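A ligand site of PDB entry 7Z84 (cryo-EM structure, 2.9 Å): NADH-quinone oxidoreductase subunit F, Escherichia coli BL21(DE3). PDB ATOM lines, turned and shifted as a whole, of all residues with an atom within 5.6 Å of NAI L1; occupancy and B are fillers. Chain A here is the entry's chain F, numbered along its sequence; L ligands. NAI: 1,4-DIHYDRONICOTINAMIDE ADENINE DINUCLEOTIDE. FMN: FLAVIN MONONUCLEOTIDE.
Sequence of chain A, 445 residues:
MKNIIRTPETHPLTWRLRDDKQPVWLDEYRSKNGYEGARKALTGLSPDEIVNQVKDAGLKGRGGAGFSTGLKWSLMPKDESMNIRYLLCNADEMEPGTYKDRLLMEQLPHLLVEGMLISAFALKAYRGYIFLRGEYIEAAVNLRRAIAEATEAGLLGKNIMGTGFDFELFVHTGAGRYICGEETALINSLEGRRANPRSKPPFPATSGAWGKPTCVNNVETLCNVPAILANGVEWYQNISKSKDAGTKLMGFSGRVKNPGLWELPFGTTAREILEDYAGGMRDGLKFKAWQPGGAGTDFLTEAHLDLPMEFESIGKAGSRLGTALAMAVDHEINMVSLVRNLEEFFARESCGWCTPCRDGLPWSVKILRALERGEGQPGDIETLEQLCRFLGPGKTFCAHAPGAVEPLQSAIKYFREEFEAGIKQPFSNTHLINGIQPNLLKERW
An oxygen (O2') of FMN L2 lies within hydrogen-bond range of an oxygen (O2N) of NAI L1, at 2.7 Å.
The backbone NH (N) of Gly 63 sits at hydrogen-bond distance from an oxygen (O1P) of FMN L2, at 2.8 Å.
An oxygen (O2D) of NAI L1 lies within hydrogen-bond range of the guanidinium group (NH1) of Arg 320, at 2.8 Å.
NZ of Lys 72 is in hydrogen-bond range of O3B of NAI L1, at 2.7 Å.
The backbone NH (N) of Glu 93 lies within hydrogen-bond range of an oxygen (O4) of FMN L2 (3.1 Å).
An oxygen (O3P) of FMN L2 sits at hydrogen-bond distance from the backbone NH (N) of Asn 218, 2.6 Å away.
NZ of Lys 200 lies within salt-bridge range of O2N of NAI L1, at 3.99 Å.
OE1 of Glu 183 sits at hydrogen-bond distance from O2B of NAI L1 (2.8 Å).
The backbone NH (N) of Arg 62 lies within hydrogen-bond range of an oxygen (O1P) of FMN L2 (3.5 Å).
OD1 of Asn 218 lies close to O2 of FMN L2 (2.9 Å).
The backbone carbonyl oxygen (O) of Gly 64 sits at hydrogen-bond distance from an oxygen (O2D) of NAI L1, 2.7 Å away.
O2P of FMN L2 is in salt-bridge range of NZ of Lys 72 (3.0 Å).
OE1 of Glu 183 is in salt-bridge range of NZ of Lys 200 (3.5 Å).
The side-chain amino group (NZ) of Lys 72 is in hydrogen-bond range of the backbone carbonyl oxygen (O) of Val 216, 2.7 Å away.
The backbone carbonyl oxygen of Glu 95 lies close to the side-chain hydroxyl of Thr 98 (3.3 Å).
The backbone NH (N) of Lys 100 sits at hydrogen-bond distance from the side-chain carboxylate (OE2) of Glu 93, at 2.5 Å.
The side-chain amide nitrogen (ND2) of Asn 218 lies close to the backbone NH (N) of Gly 63 (3.5 Å).
The side-chain hydroxyl (OH) of Tyr 178 is in hydrogen-bond range of the side-chain carboxylate (OE1) of Glu 95, 3.1 Å away.
The side-chain hydroxyl (OG1) of Thr 323 is in hydrogen-bond range of the side-chain hydroxyl (OG1) of Thr 98 (3.5 Å).
The side-chain hydroxyl (OG1) of Thr 323 sits at hydrogen-bond distance from the backbone carbonyl oxygen (O) of Gly 293, at 3.1 Å.
O of Gly 63 sits close to O7N of NAI L1 (2.9 Å).
The backbone NH of Glu 95 lies close to a nitrogen (N7N) of NAI L1.
Merely in contact with NAI L1: Tyr 178 (3.2 Å), Phe 67 (3.2 Å), Ala 65 (3.4 Å), Phe 203 (3.4 Å), Thr 323 (3.5 Å), Leu 75 (3.6 Å), Met 94 (3.7 Å), Ala 399 (3.7 Å), Gly 322 (3.8 Å), Glu 93 (3.8 Å) and Glu 182 (3.96 Å).
Of the 25 residues printed, 18 come within 4 Å of NAI L1.
Along chain A the residues within 4 Å of NAI L1 span positions 63 to 399.
The nearest printed residue that does not touch NAI L1 is Val 216 (4.4 Å).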
ATOM      1  N   ARG A  62      -7.635  10.457   5.528  1.00  0.00           N
ATOM      2  CA  ARG A  62      -7.158  11.547   4.688  1.00  0.00           C
ATOM      3  C   ARG A  62      -5.713  11.374   4.254  1.00  0.00           C
ATOM      4  O   ARG A  62      -5.167  12.271   3.613  1.00  0.00           O
ATOM      5  CB  ARG A  62      -7.317  12.875   5.414  1.00  0.00           C
ATOM      6  CG  ARG A  62      -8.737  13.156   5.896  1.00  0.00           C
ATOM      7  CD  ARG A  62      -9.685  13.292   4.736  1.00  0.00           C
ATOM      8  NE  ARG A  62     -10.833  14.128   5.064  1.00  0.00           N
ATOM      9  CZ  ARG A  62     -12.057  13.675   5.284  1.00  0.00           C
ATOM     10  NH1 ARG A  62     -12.332  12.384   5.215  1.00  0.00           N
ATOM     11  NH2 ARG A  62     -13.029  14.529   5.584  1.00  0.00           N
ATOM     12  N   GLY A  63      -5.076  10.246   4.606  1.00  0.00           N
ATOM     13  CA  GLY A  63      -3.715  10.004   4.155  1.00  0.00           C
ATOM     14  C   GLY A  63      -3.607   9.799   2.659  1.00  0.00           C
ATOM     15  O   GLY A  63      -2.593  10.159   2.051  1.00  0.00           O
ATOM     16  N   GLY A  64      -4.641   9.232   2.048  1.00  0.00           N
ATOM     17  CA  GLY A  64      -4.627   9.012   0.615  1.00  0.00           C
ATOM     18  C   GLY A  64      -5.271   7.702   0.198  1.00  0.00           C
ATOM     19  O   GLY A  64      -5.443   7.442  -0.996  1.00  0.00           O
ATOM     20  N   ALA A  65      -5.644   6.874   1.169  1.00  0.00           N
ATOM     21  CA  ALA A  65      -6.242   5.579   0.879  1.00  0.00           C
ATOM     22  C   ALA A  65      -7.748   5.551   1.089  1.00  0.00           C
ATOM     23  O   ALA A  65      -8.429   4.728   0.478  1.00  0.00           O
ATOM     24  CB  ALA A  65      -5.602   4.490   1.736  1.00  0.00           C
ATOM     25  N   PHE A  67      -9.527   4.723   3.758  1.00  0.00           N
ATOM     26  CA  PHE A  67     -10.079   3.766   4.704  1.00  0.00           C
ATOM     27  C   PHE A  67     -10.812   4.499   5.818  1.00  0.00           C
ATOM     28  O   PHE A  67     -10.378   5.560   6.280  1.00  0.00           O
ATOM     29  CB  PHE A  67      -8.957   2.895   5.286  1.00  0.00           C
ATOM     30  CG  PHE A  67      -9.442   1.647   5.960  1.00  0.00           C
ATOM     31  CD1 PHE A  67      -9.948   0.589   5.204  1.00  0.00           C
ATOM     32  CD2 PHE A  67      -9.412   1.526   7.337  1.00  0.00           C
ATOM     33  CE1 PHE A  67     -10.393  -0.556   5.815  1.00  0.00           C
ATOM     34  CE2 PHE A  67      -9.862   0.369   7.953  1.00  0.00           C
ATOM     35  CZ  PHE A  67     -10.352  -0.670   7.197  1.00  0.00           C
ATOM     36  N   LYS A  72     -11.252   1.365  11.584  1.00  0.00           N
ATOM     37  CA  LYS A  72      -9.871   1.145  12.008  1.00  0.00           C
ATOM     38  C   LYS A  72      -9.748   1.238  13.528  1.00  0.00           C
ATOM     39  O   LYS A  72      -8.953   0.517  14.138  1.00  0.00           O
ATOM     40  CB  LYS A  72      -8.945   2.160  11.347  1.00  0.00           C
ATOM     41  CG  LYS A  72      -7.475   1.786  11.425  1.00  0.00           C
ATOM     42  CD  LYS A  72      -6.591   3.008  11.364  1.00  0.00           C
ATOM     43  CE  LYS A  72      -6.676   3.685  10.012  1.00  0.00           C
ATOM     44  NZ  LYS A  72      -5.454   4.487   9.735  1.00  0.00           N
ATOM     45  N   LEU A  75     -11.233  -2.093  15.252  1.00  0.00           N
ATOM     46  CA  LEU A  75     -10.449  -3.324  15.222  1.00  0.00           C
ATOM     47  C   LEU A  75      -9.358  -3.363  16.285  1.00  0.00           C
ATOM     48  O   LEU A  75      -8.529  -4.270  16.265  1.00  0.00           O
ATOM     49  CB  LEU A  75      -9.836  -3.552  13.836  1.00  0.00           C
ATOM     50  CG  LEU A  75     -10.827  -3.609  12.678  1.00  0.00           C
ATOM     51  CD1 LEU A  75     -10.101  -3.818  11.367  1.00  0.00           C
ATOM     52  CD2 LEU A  75     -11.865  -4.693  12.907  1.00  0.00           C
ATOM     53  N   GLU A  93       4.218  13.325   5.460  1.00  0.00           N
ATOM     54  CA  GLU A  93       3.755  14.082   4.289  1.00  0.00           C
ATOM     55  C   GLU A  93       4.878  14.291   3.273  1.00  0.00           C
ATOM     56  O   GLU A  93       5.190  15.415   2.881  1.00  0.00           O
ATOM     57  CB  GLU A  93       3.129  15.411   4.695  1.00  0.00           C
ATOM     58  CG  GLU A  93       2.070  15.910   3.731  1.00  0.00           C
ATOM     59  CD  GLU A  93       1.926  17.416   3.768  1.00  0.00           C
ATOM     60  OE1 GLU A  93       2.890  18.108   4.144  1.00  0.00           O
ATOM     61  OE2 GLU A  93       0.827  17.909   3.417  1.00  0.00           O
ATOM     62  N   MET A  94       5.486  13.194   2.863  1.00  0.00           N
ATOM     63  CA  MET A  94       6.642  13.242   1.985  1.00  0.00           C
ATOM     64  C   MET A  94       6.282  13.071   0.510  1.00  0.00           C
ATOM     65  O   MET A  94       7.189  13.035  -0.328  1.00  0.00           O
ATOM     66  CB  MET A  94       7.660  12.166   2.400  1.00  0.00           C
ATOM     67  CG  MET A  94       8.729  12.656   3.347  1.00  0.00           C
ATOM     68  SD  MET A  94      10.250  13.091   2.484  1.00  0.00           S
ATOM     69  CE  MET A  94      11.405  13.103   3.843  1.00  0.00           C
ATOM     70  N   GLU A  95       5.008  12.983   0.190  1.00  0.00           N
ATOM     71  CA  GLU A  95       4.589  12.842  -1.205  1.00  0.00           C
ATOM     72  C   GLU A  95       4.797  14.154  -1.950  1.00  0.00           C
ATOM     73  O   GLU A  95       4.409  15.213  -1.445  1.00  0.00           O
ATOM     74  CB  GLU A  95       3.128  12.423  -1.297  1.00  0.00           C
ATOM     75  CG  GLU A  95       2.599  12.282  -2.710  1.00  0.00           C
ATOM     76  CD  GLU A  95       2.681  10.866  -3.225  1.00  0.00           C
ATOM     77  OE1 GLU A  95       3.812  10.342  -3.368  1.00  0.00           O
ATOM     78  OE2 GLU A  95       1.615  10.262  -3.491  1.00  0.00           O
ATOM     79  N   THR A  98       2.147  17.344  -2.212  1.00  0.00           N
ATOM     80  CA  THR A  98       1.352  17.389  -0.993  1.00  0.00           C
ATOM     81  C   THR A  98       1.953  18.406  -0.032  1.00  0.00           C
ATOM     82  O   THR A  98       3.129  18.291   0.342  1.00  0.00           O
ATOM     83  CB  THR A  98       1.257  16.013  -0.337  1.00  0.00           C
ATOM     84  OG1 THR A  98       1.115  15.016  -1.352  1.00  0.00           O
ATOM     85  CG2 THR A  98       0.070  15.955   0.597  1.00  0.00           C
ATOM     86  N   LYS A 100      -0.455  19.881   2.545  1.00  0.00           N
ATOM     87  CA  LYS A 100      -1.621  20.220   3.352  1.00  0.00           C
ATOM     88  C   LYS A 100      -1.333  20.108   4.841  1.00  0.00           C
ATOM     89  O   LYS A 100      -1.824  20.916   5.632  1.00  0.00           O
ATOM     90  CB  LYS A 100      -2.802  19.347   2.949  1.00  0.00           C
ATOM     91  CG  LYS A 100      -2.491  17.869   2.816  1.00  0.00           C
ATOM     92  CD  LYS A 100      -3.721  17.079   2.423  1.00  0.00           C
ATOM     93  CE  LYS A 100      -3.477  15.589   2.511  1.00  0.00           C
ATOM     94  NZ  LYS A 100      -3.285  15.155   3.924  1.00  0.00           N
ATOM     95  N   TYR A 178      11.377   9.062   2.544  1.00  0.00           N
ATOM     96  CA  TYR A 178       9.997   9.074   2.074  1.00  0.00           C
ATOM     97  C   TYR A 178       9.222   7.847   2.521  1.00  0.00           C
ATOM     98  O   TYR A 178       8.023   7.938   2.785  1.00  0.00           O
ATOM     99  CB  TYR A 178       9.975   9.199   0.549  1.00  0.00           C
ATOM    100  CG  TYR A 178       8.668   8.831  -0.113  1.00  0.00           C
ATOM    101  CD1 TYR A 178       7.596   9.715  -0.124  1.00  0.00           C
ATOM    102  CD2 TYR A 178       8.510   7.615  -0.764  1.00  0.00           C
ATOM    103  CE1 TYR A 178       6.403   9.392  -0.743  1.00  0.00           C
ATOM    104  CE2 TYR A 178       7.321   7.282  -1.381  1.00  0.00           C
ATOM    105  CZ  TYR A 178       6.277   8.176  -1.369  1.00  0.00           C
ATOM    106  OH  TYR A 178       5.097   7.847  -1.990  1.00  0.00           O
ATOM    107  N   GLU A 182       4.871   5.302   5.233  1.00  0.00           N
ATOM    108  CA  GLU A 182       4.167   4.026   5.327  1.00  0.00           C
ATOM    109  C   GLU A 182       4.047   3.629   6.790  1.00  0.00           C
ATOM    110  O   GLU A 182       5.027   3.667   7.525  1.00  0.00           O
ATOM    111  CB  GLU A 182       4.919   2.943   4.544  1.00  0.00           C
ATOM    112  CG  GLU A 182       4.025   1.938   3.860  1.00  0.00           C
ATOM    113  CD  GLU A 182       3.675   0.759   4.739  1.00  0.00           C
ATOM    114  OE1 GLU A 182       4.275   0.629   5.826  1.00  0.00           O
ATOM    115  OE2 GLU A 182       2.785  -0.027   4.351  1.00  0.00           O
ATOM    116  N   GLU A 183       2.825   3.245   7.192  1.00  0.00           N
ATOM    117  CA  GLU A 183       2.494   3.171   8.614  1.00  0.00           C
ATOM    118  C   GLU A 183       3.304   2.102   9.344  1.00  0.00           C
ATOM    119  O   GLU A 183       3.709   2.300  10.496  1.00  0.00           O
ATOM    120  CB  GLU A 183       0.993   2.942   8.797  1.00  0.00           C
ATOM    121  CG  GLU A 183       0.496   1.618   8.250  1.00  0.00           C
ATOM    122  CD  GLU A 183      -0.747   1.138   8.942  1.00  0.00           C
ATOM    123  OE1 GLU A 183      -1.520   0.412   8.301  1.00  0.00           O
ATOM    124  OE2 GLU A 183      -0.957   1.497  10.120  1.00  0.00           O
ATOM    125  N   LYS A 200       1.106  -7.311   6.391  1.00  0.00           N
ATOM    126  CA  LYS A 200      -0.164  -7.329   7.095  1.00  0.00           C
ATOM    127  C   LYS A 200      -1.065  -8.378   6.465  1.00  0.00           C
ATOM    128  O   LYS A 200      -1.163  -8.441   5.237  1.00  0.00           O
ATOM    129  CB  LYS A 200      -0.829  -5.950   7.045  1.00  0.00           C
ATOM    130  CG  LYS A 200       0.020  -4.837   7.628  1.00  0.00           C
ATOM    131  CD  LYS A 200      -0.574  -3.472   7.344  1.00  0.00           C
ATOM    132  CE  LYS A 200      -0.459  -3.103   5.872  1.00  0.00           C
ATOM    133  NZ  LYS A 200      -0.915  -1.708   5.620  1.00  0.00           N
ATOM    134  N   PHE A 203      -2.205  -6.504  11.389  1.00  0.00           N
ATOM    135  CA  PHE A 203      -2.299  -5.067  11.231  1.00  0.00           C
ATOM    136  C   PHE A 203      -1.809  -4.378  12.501  1.00  0.00           C
ATOM    137  O   PHE A 203      -1.757  -4.998  13.560  1.00  0.00           O
ATOM    138  CB  PHE A 203      -3.736  -4.685  10.898  1.00  0.00           C
ATOM    139  CG  PHE A 203      -4.163  -5.121   9.528  1.00  0.00           C
ATOM    140  CD1 PHE A 203      -3.912  -4.323   8.422  1.00  0.00           C
ATOM    141  CD2 PHE A 203      -4.781  -6.350   9.338  1.00  0.00           C
ATOM    142  CE1 PHE A 203      -4.290  -4.729   7.150  1.00  0.00           C
ATOM    143  CE2 PHE A 203      -5.152  -6.760   8.078  1.00  0.00           C
ATOM    144  CZ  PHE A 203      -4.912  -5.953   6.981  1.00  0.00           C
ATOM    145  N   PRO A 204      -1.410  -3.098  12.412  1.00  0.00           N
ATOM    146  CA  PRO A 204      -0.907  -2.401  13.609  1.00  0.00           C
ATOM    147  C   PRO A 204      -1.913  -2.279  14.736  1.00  0.00           C
ATOM    148  O   PRO A 204      -1.499  -2.078  15.884  1.00  0.00           O
ATOM    149  CB  PRO A 204      -0.505  -1.027  13.069  1.00  0.00           C
ATOM    150  CG  PRO A 204      -0.119  -1.300  11.668  1.00  0.00           C
ATOM    151  CD  PRO A 204      -1.087  -2.348  11.186  1.00  0.00           C
ATOM    152  N   VAL A 216      -2.463   4.350  13.689  1.00  0.00           N
ATOM    153  CA  VAL A 216      -1.776   5.396  12.939  1.00  0.00           C
ATOM    154  C   VAL A 216      -2.798   6.145  12.096  1.00  0.00           C
ATOM    155  O   VAL A 216      -3.544   5.519  11.328  1.00  0.00           O
ATOM    156  CB  VAL A 216      -0.654   4.819  12.065  1.00  0.00           C
ATOM    157  CG1 VAL A 216       0.137   5.932  11.407  1.00  0.00           C
ATOM    158  CG2 VAL A 216       0.248   3.916  12.891  1.00  0.00           C
ATOM    159  N   ASN A 218      -3.536  10.064   9.843  1.00  0.00           N
ATOM    160  CA  ASN A 218      -2.959  11.264   9.244  1.00  0.00           C
ATOM    161  C   ASN A 218      -3.282  12.494  10.096  1.00  0.00           C
ATOM    162  O   ASN A 218      -4.124  12.456  11.004  1.00  0.00           O
ATOM    163  CB  ASN A 218      -3.470  11.438   7.817  1.00  0.00           C
ATOM    164  CG  ASN A 218      -2.603  12.375   6.992  1.00  0.00           C
ATOM    165  OD1 ASN A 218      -1.482  12.709   7.380  1.00  0.00           O
ATOM    166  ND2 ASN A 218      -3.127  12.817   5.866  1.00  0.00           N
ATOM    167  N   GLY A 293      -3.992  13.344  -7.012  1.00  0.00           N
ATOM    168  CA  GLY A 293      -3.652  13.206  -5.614  1.00  0.00           C
ATOM    169  C   GLY A 293      -2.176  13.046  -5.294  1.00  0.00           C
ATOM    170  O   GLY A 293      -1.831  12.305  -4.378  1.00  0.00           O
ATOM    171  N   ARG A 320      -6.506   7.731  -8.838  1.00  0.00           N
ATOM    172  CA  ARG A 320      -6.816   7.725  -7.415  1.00  0.00           C
ATOM    173  C   ARG A 320      -7.046   9.141  -6.931  1.00  0.00           C
ATOM    174  O   ARG A 320      -6.428  10.094  -7.425  1.00  0.00           O
ATOM    175  CB  ARG A 320      -5.700   7.074  -6.591  1.00  0.00           C
ATOM    176  CG  ARG A 320      -5.548   5.577  -6.800  1.00  0.00           C
ATOM    177  CD  ARG A 320      -4.660   4.984  -5.722  1.00  0.00           C
ATOM    178  NE  ARG A 320      -3.246   5.235  -5.960  1.00  0.00           N
ATOM    179  CZ  ARG A 320      -2.532   6.174  -5.360  1.00  0.00           C
ATOM    180  NH1 ARG A 320      -3.084   7.009  -4.498  1.00  0.00           N
ATOM    181  NH2 ARG A 320      -1.236   6.278  -5.629  1.00  0.00           N
ATOM    182  N   GLY A 322      -6.291  10.065  -3.824  1.00  0.00           N
ATOM    183  CA  GLY A 322      -5.028  10.327  -3.140  1.00  0.00           C
ATOM    184  C   GLY A 322      -5.152  11.377  -2.061  1.00  0.00           C
ATOM    185  O   GLY A 322      -6.097  11.384  -1.257  1.00  0.00           O
ATOM    186  N   THR A 323      -4.196  12.303  -2.037  1.00  0.00           N
ATOM    187  CA  THR A 323      -4.186  13.417  -1.106  1.00  0.00           C
ATOM    188  C   THR A 323      -5.055  14.581  -1.583  1.00  0.00           C
ATOM    189  O   THR A 323      -5.115  15.602  -0.886  1.00  0.00           O
ATOM    190  CB  THR A 323      -2.762  13.909  -0.869  1.00  0.00           C
ATOM    191  OG1 THR A 323      -2.217  14.421  -2.094  1.00  0.00           O
ATOM    192  CG2 THR A 323      -1.884  12.765  -0.380  1.00  0.00           C
ATOM    193  N   ALA A 399       3.014  -0.768  -0.928  1.00  0.00           N
ATOM    194  CA  ALA A 399       2.300  -0.059  -1.974  1.00  0.00           C
ATOM    195  C   ALA A 399       3.089   1.110  -2.555  1.00  0.00           C
ATOM    196  O   ALA A 399       2.506   1.977  -3.211  1.00  0.00           O
ATOM    197  CB  ALA A 399       0.950   0.436  -1.465  1.00  0.00           C
HETATM  198  PA  NAI L   1      -4.028   0.523   2.584  1.00  0.00           P
HETATM  199  O1A NAI L   1      -5.070   1.167   1.767  1.00  0.00           O
HETATM  200  O2A NAI L   1      -4.077  -0.995   2.622  1.00  0.00           O
HETATM  201  O5B NAI L   1      -4.099   1.012   4.119  1.00  0.00           O
HETATM  202  C5B NAI L   1      -4.658   2.284   4.499  1.00  0.00           C
HETATM  203  C4B NAI L   1      -5.197   2.176   5.909  1.00  0.00           C
HETATM  204  O4B NAI L   1      -6.253   1.185   5.947  1.00  0.00           O
HETATM  205  C3B NAI L   1      -4.172   1.782   6.969  1.00  0.00           C
HETATM  206  O3B NAI L   1      -4.259   2.617   8.118  1.00  0.00           O
HETATM  207  C2B NAI L   1      -4.532   0.323   7.280  1.00  0.00           C
HETATM  208  O2B NAI L   1      -4.242  -0.015   8.629  1.00  0.00           O
HETATM  209  C1B NAI L   1      -6.043   0.317   7.037  1.00  0.00           C
HETATM  210  N9A NAI L   1      -6.576  -0.997   6.696  1.00  0.00           N
HETATM  211  C8A NAI L   1      -6.872  -1.469   5.454  1.00  0.00           C
HETATM  212  N7A NAI L   1      -7.354  -2.694   5.440  1.00  0.00           N
HETATM  213  C5A NAI L   1      -7.378  -3.046   6.783  1.00  0.00           C
HETATM  214  C6A NAI L   1      -7.781  -4.209   7.457  1.00  0.00           C
HETATM  215  N6A NAI L   1      -8.266  -5.295   6.841  1.00  0.00           N
HETATM  216  N1A NAI L   1      -7.661  -4.240   8.797  1.00  0.00           N
HETATM  217  C2A NAI L   1      -7.170  -3.159   9.424  1.00  0.00           C
HETATM  218  N3A NAI L   1      -6.770  -2.010   8.901  1.00  0.00           N
HETATM  219  C4A NAI L   1      -6.895  -2.011   7.576  1.00  0.00           C
HETATM  220  O3  NAI L   1      -2.570   0.920   2.075  1.00  0.00           O
HETATM  221  PN  NAI L   1      -1.393   1.855   2.609  1.00  0.00           P
HETATM  222  O1N NAI L   1      -0.104   1.323   1.997  1.00  0.00           O
HETATM  223  O2N NAI L   1      -1.368   1.943   4.077  1.00  0.00           O
HETATM  224  O5D NAI L   1      -1.654   3.282   1.929  1.00  0.00           O
HETATM  225  C5D NAI L   1      -1.725   3.461   0.504  1.00  0.00           C
HETATM  226  C4D NAI L   1      -2.127   4.880   0.207  1.00  0.00           C
HETATM  227  O4D NAI L   1      -1.130   5.781   0.688  1.00  0.00           O
HETATM  228  C3D NAI L   1      -2.282   5.216  -1.285  1.00  0.00           C
HETATM  229  O3D NAI L   1      -3.634   5.084  -1.702  1.00  0.00           O
HETATM  230  C2D NAI L   1      -1.792   6.676  -1.383  1.00  0.00           C
HETATM  231  O2D NAI L   1      -2.846   7.554  -1.784  1.00  0.00           O
HETATM  232  C1D NAI L   1      -1.321   7.008   0.031  1.00  0.00           C
HETATM  233  N1N NAI L   1      -0.059   7.749   0.058  1.00  0.00           N
HETATM  234  C2N NAI L   1       0.061   8.936   0.787  1.00  0.00           C
HETATM  235  C3N NAI L   1       1.194   9.658   0.843  1.00  0.00           C
HETATM  236  C7N NAI L   1       1.174  10.904   1.647  1.00  0.00           C
HETATM  237  O7N NAI L   1       0.111  11.318   2.120  1.00  0.00           O
HETATM  238  N7N NAI L   1       2.318  11.542   1.825  1.00  0.00           N
HETATM  239  C4N NAI L   1       2.418   9.208   0.112  1.00  0.00           C
HETATM  240  C5N NAI L   1       2.188   7.948  -0.648  1.00  0.00           C
HETATM  241  C6N NAI L   1       1.025   7.310  -0.643  1.00  0.00           C
HETATM  242  N1  FMN L   2       0.313   8.613   5.017  1.00  0.00           N
HETATM  243  C2  FMN L   2       0.548   9.842   5.589  1.00  0.00           C
HETATM  244  O2  FMN L   2      -0.301  10.341   6.308  1.00  0.00           O
HETATM  245  N3  FMN L   2       1.735  10.500   5.347  1.00  0.00           N
HETATM  246  C4  FMN L   2       2.689   9.916   4.527  1.00  0.00           C
HETATM  247  O4  FMN L   2       3.741  10.506   4.314  1.00  0.00           O
HETATM  248  C4A FMN L   2       2.445   8.684   3.959  1.00  0.00           C
HETATM  249  N5  FMN L   2       3.385   8.106   3.140  1.00  0.00           N
HETATM  250  C5A FMN L   2       3.145   6.865   2.574  1.00  0.00           C
HETATM  251  C6  FMN L   2       4.104   6.309   1.763  1.00  0.00           C
HETATM  252  C7  FMN L   2       3.888   5.074   1.178  1.00  0.00           C
HETATM  253  C7M FMN L   2       4.938   4.472   0.298  1.00  0.00           C
HETATM  254  C8  FMN L   2       2.695   4.400   1.416  1.00  0.00           C
HETATM  255  C8M FMN L   2       2.441   3.063   0.783  1.00  0.00           C
HETATM  256  C9  FMN L   2       1.726   4.965   2.237  1.00  0.00           C
HETATM  257  C9A FMN L   2       1.950   6.203   2.819  1.00  0.00           C
HETATM  258  N10 FMN L   2       0.996   6.787   3.639  1.00  0.00           N
HETATM  259  C10 FMN L   2       1.249   8.023   4.204  1.00  0.00           C
HETATM  260  C1' FMN L   2      -0.309   6.113   3.938  1.00  0.00           C
HETATM  261  C2' FMN L   2      -0.199   5.303   5.229  1.00  0.00           C
HETATM  262  O2' FMN L   2       0.164   3.973   4.932  1.00  0.00           O
HETATM  263  C3' FMN L   2      -1.509   5.305   6.024  1.00  0.00           C
HETATM  264  O3' FMN L   2      -2.584   5.173   5.129  1.00  0.00           O
HETATM  265  C4' FMN L   2      -1.641   6.597   6.814  1.00  0.00           C
HETATM  266  O4' FMN L   2      -0.420   6.892   7.450  1.00  0.00           O
HETATM  267  C5' FMN L   2      -2.743   6.557   7.865  1.00  0.00           C
HETATM  268  O5' FMN L   2      -3.982   6.230   7.269  1.00  0.00           O
HETATM  269  P   FMN L   2      -5.203   7.257   7.357  1.00  0.00           P
HETATM  270  O1P FMN L   2      -5.410   7.849   5.992  1.00  0.00           O
HETATM  271  O2P FMN L   2      -6.458   6.551   7.813  1.00  0.00           O
HETATM  272  O3P FMN L   2      -4.884   8.370   8.324  1.00  0.00           O
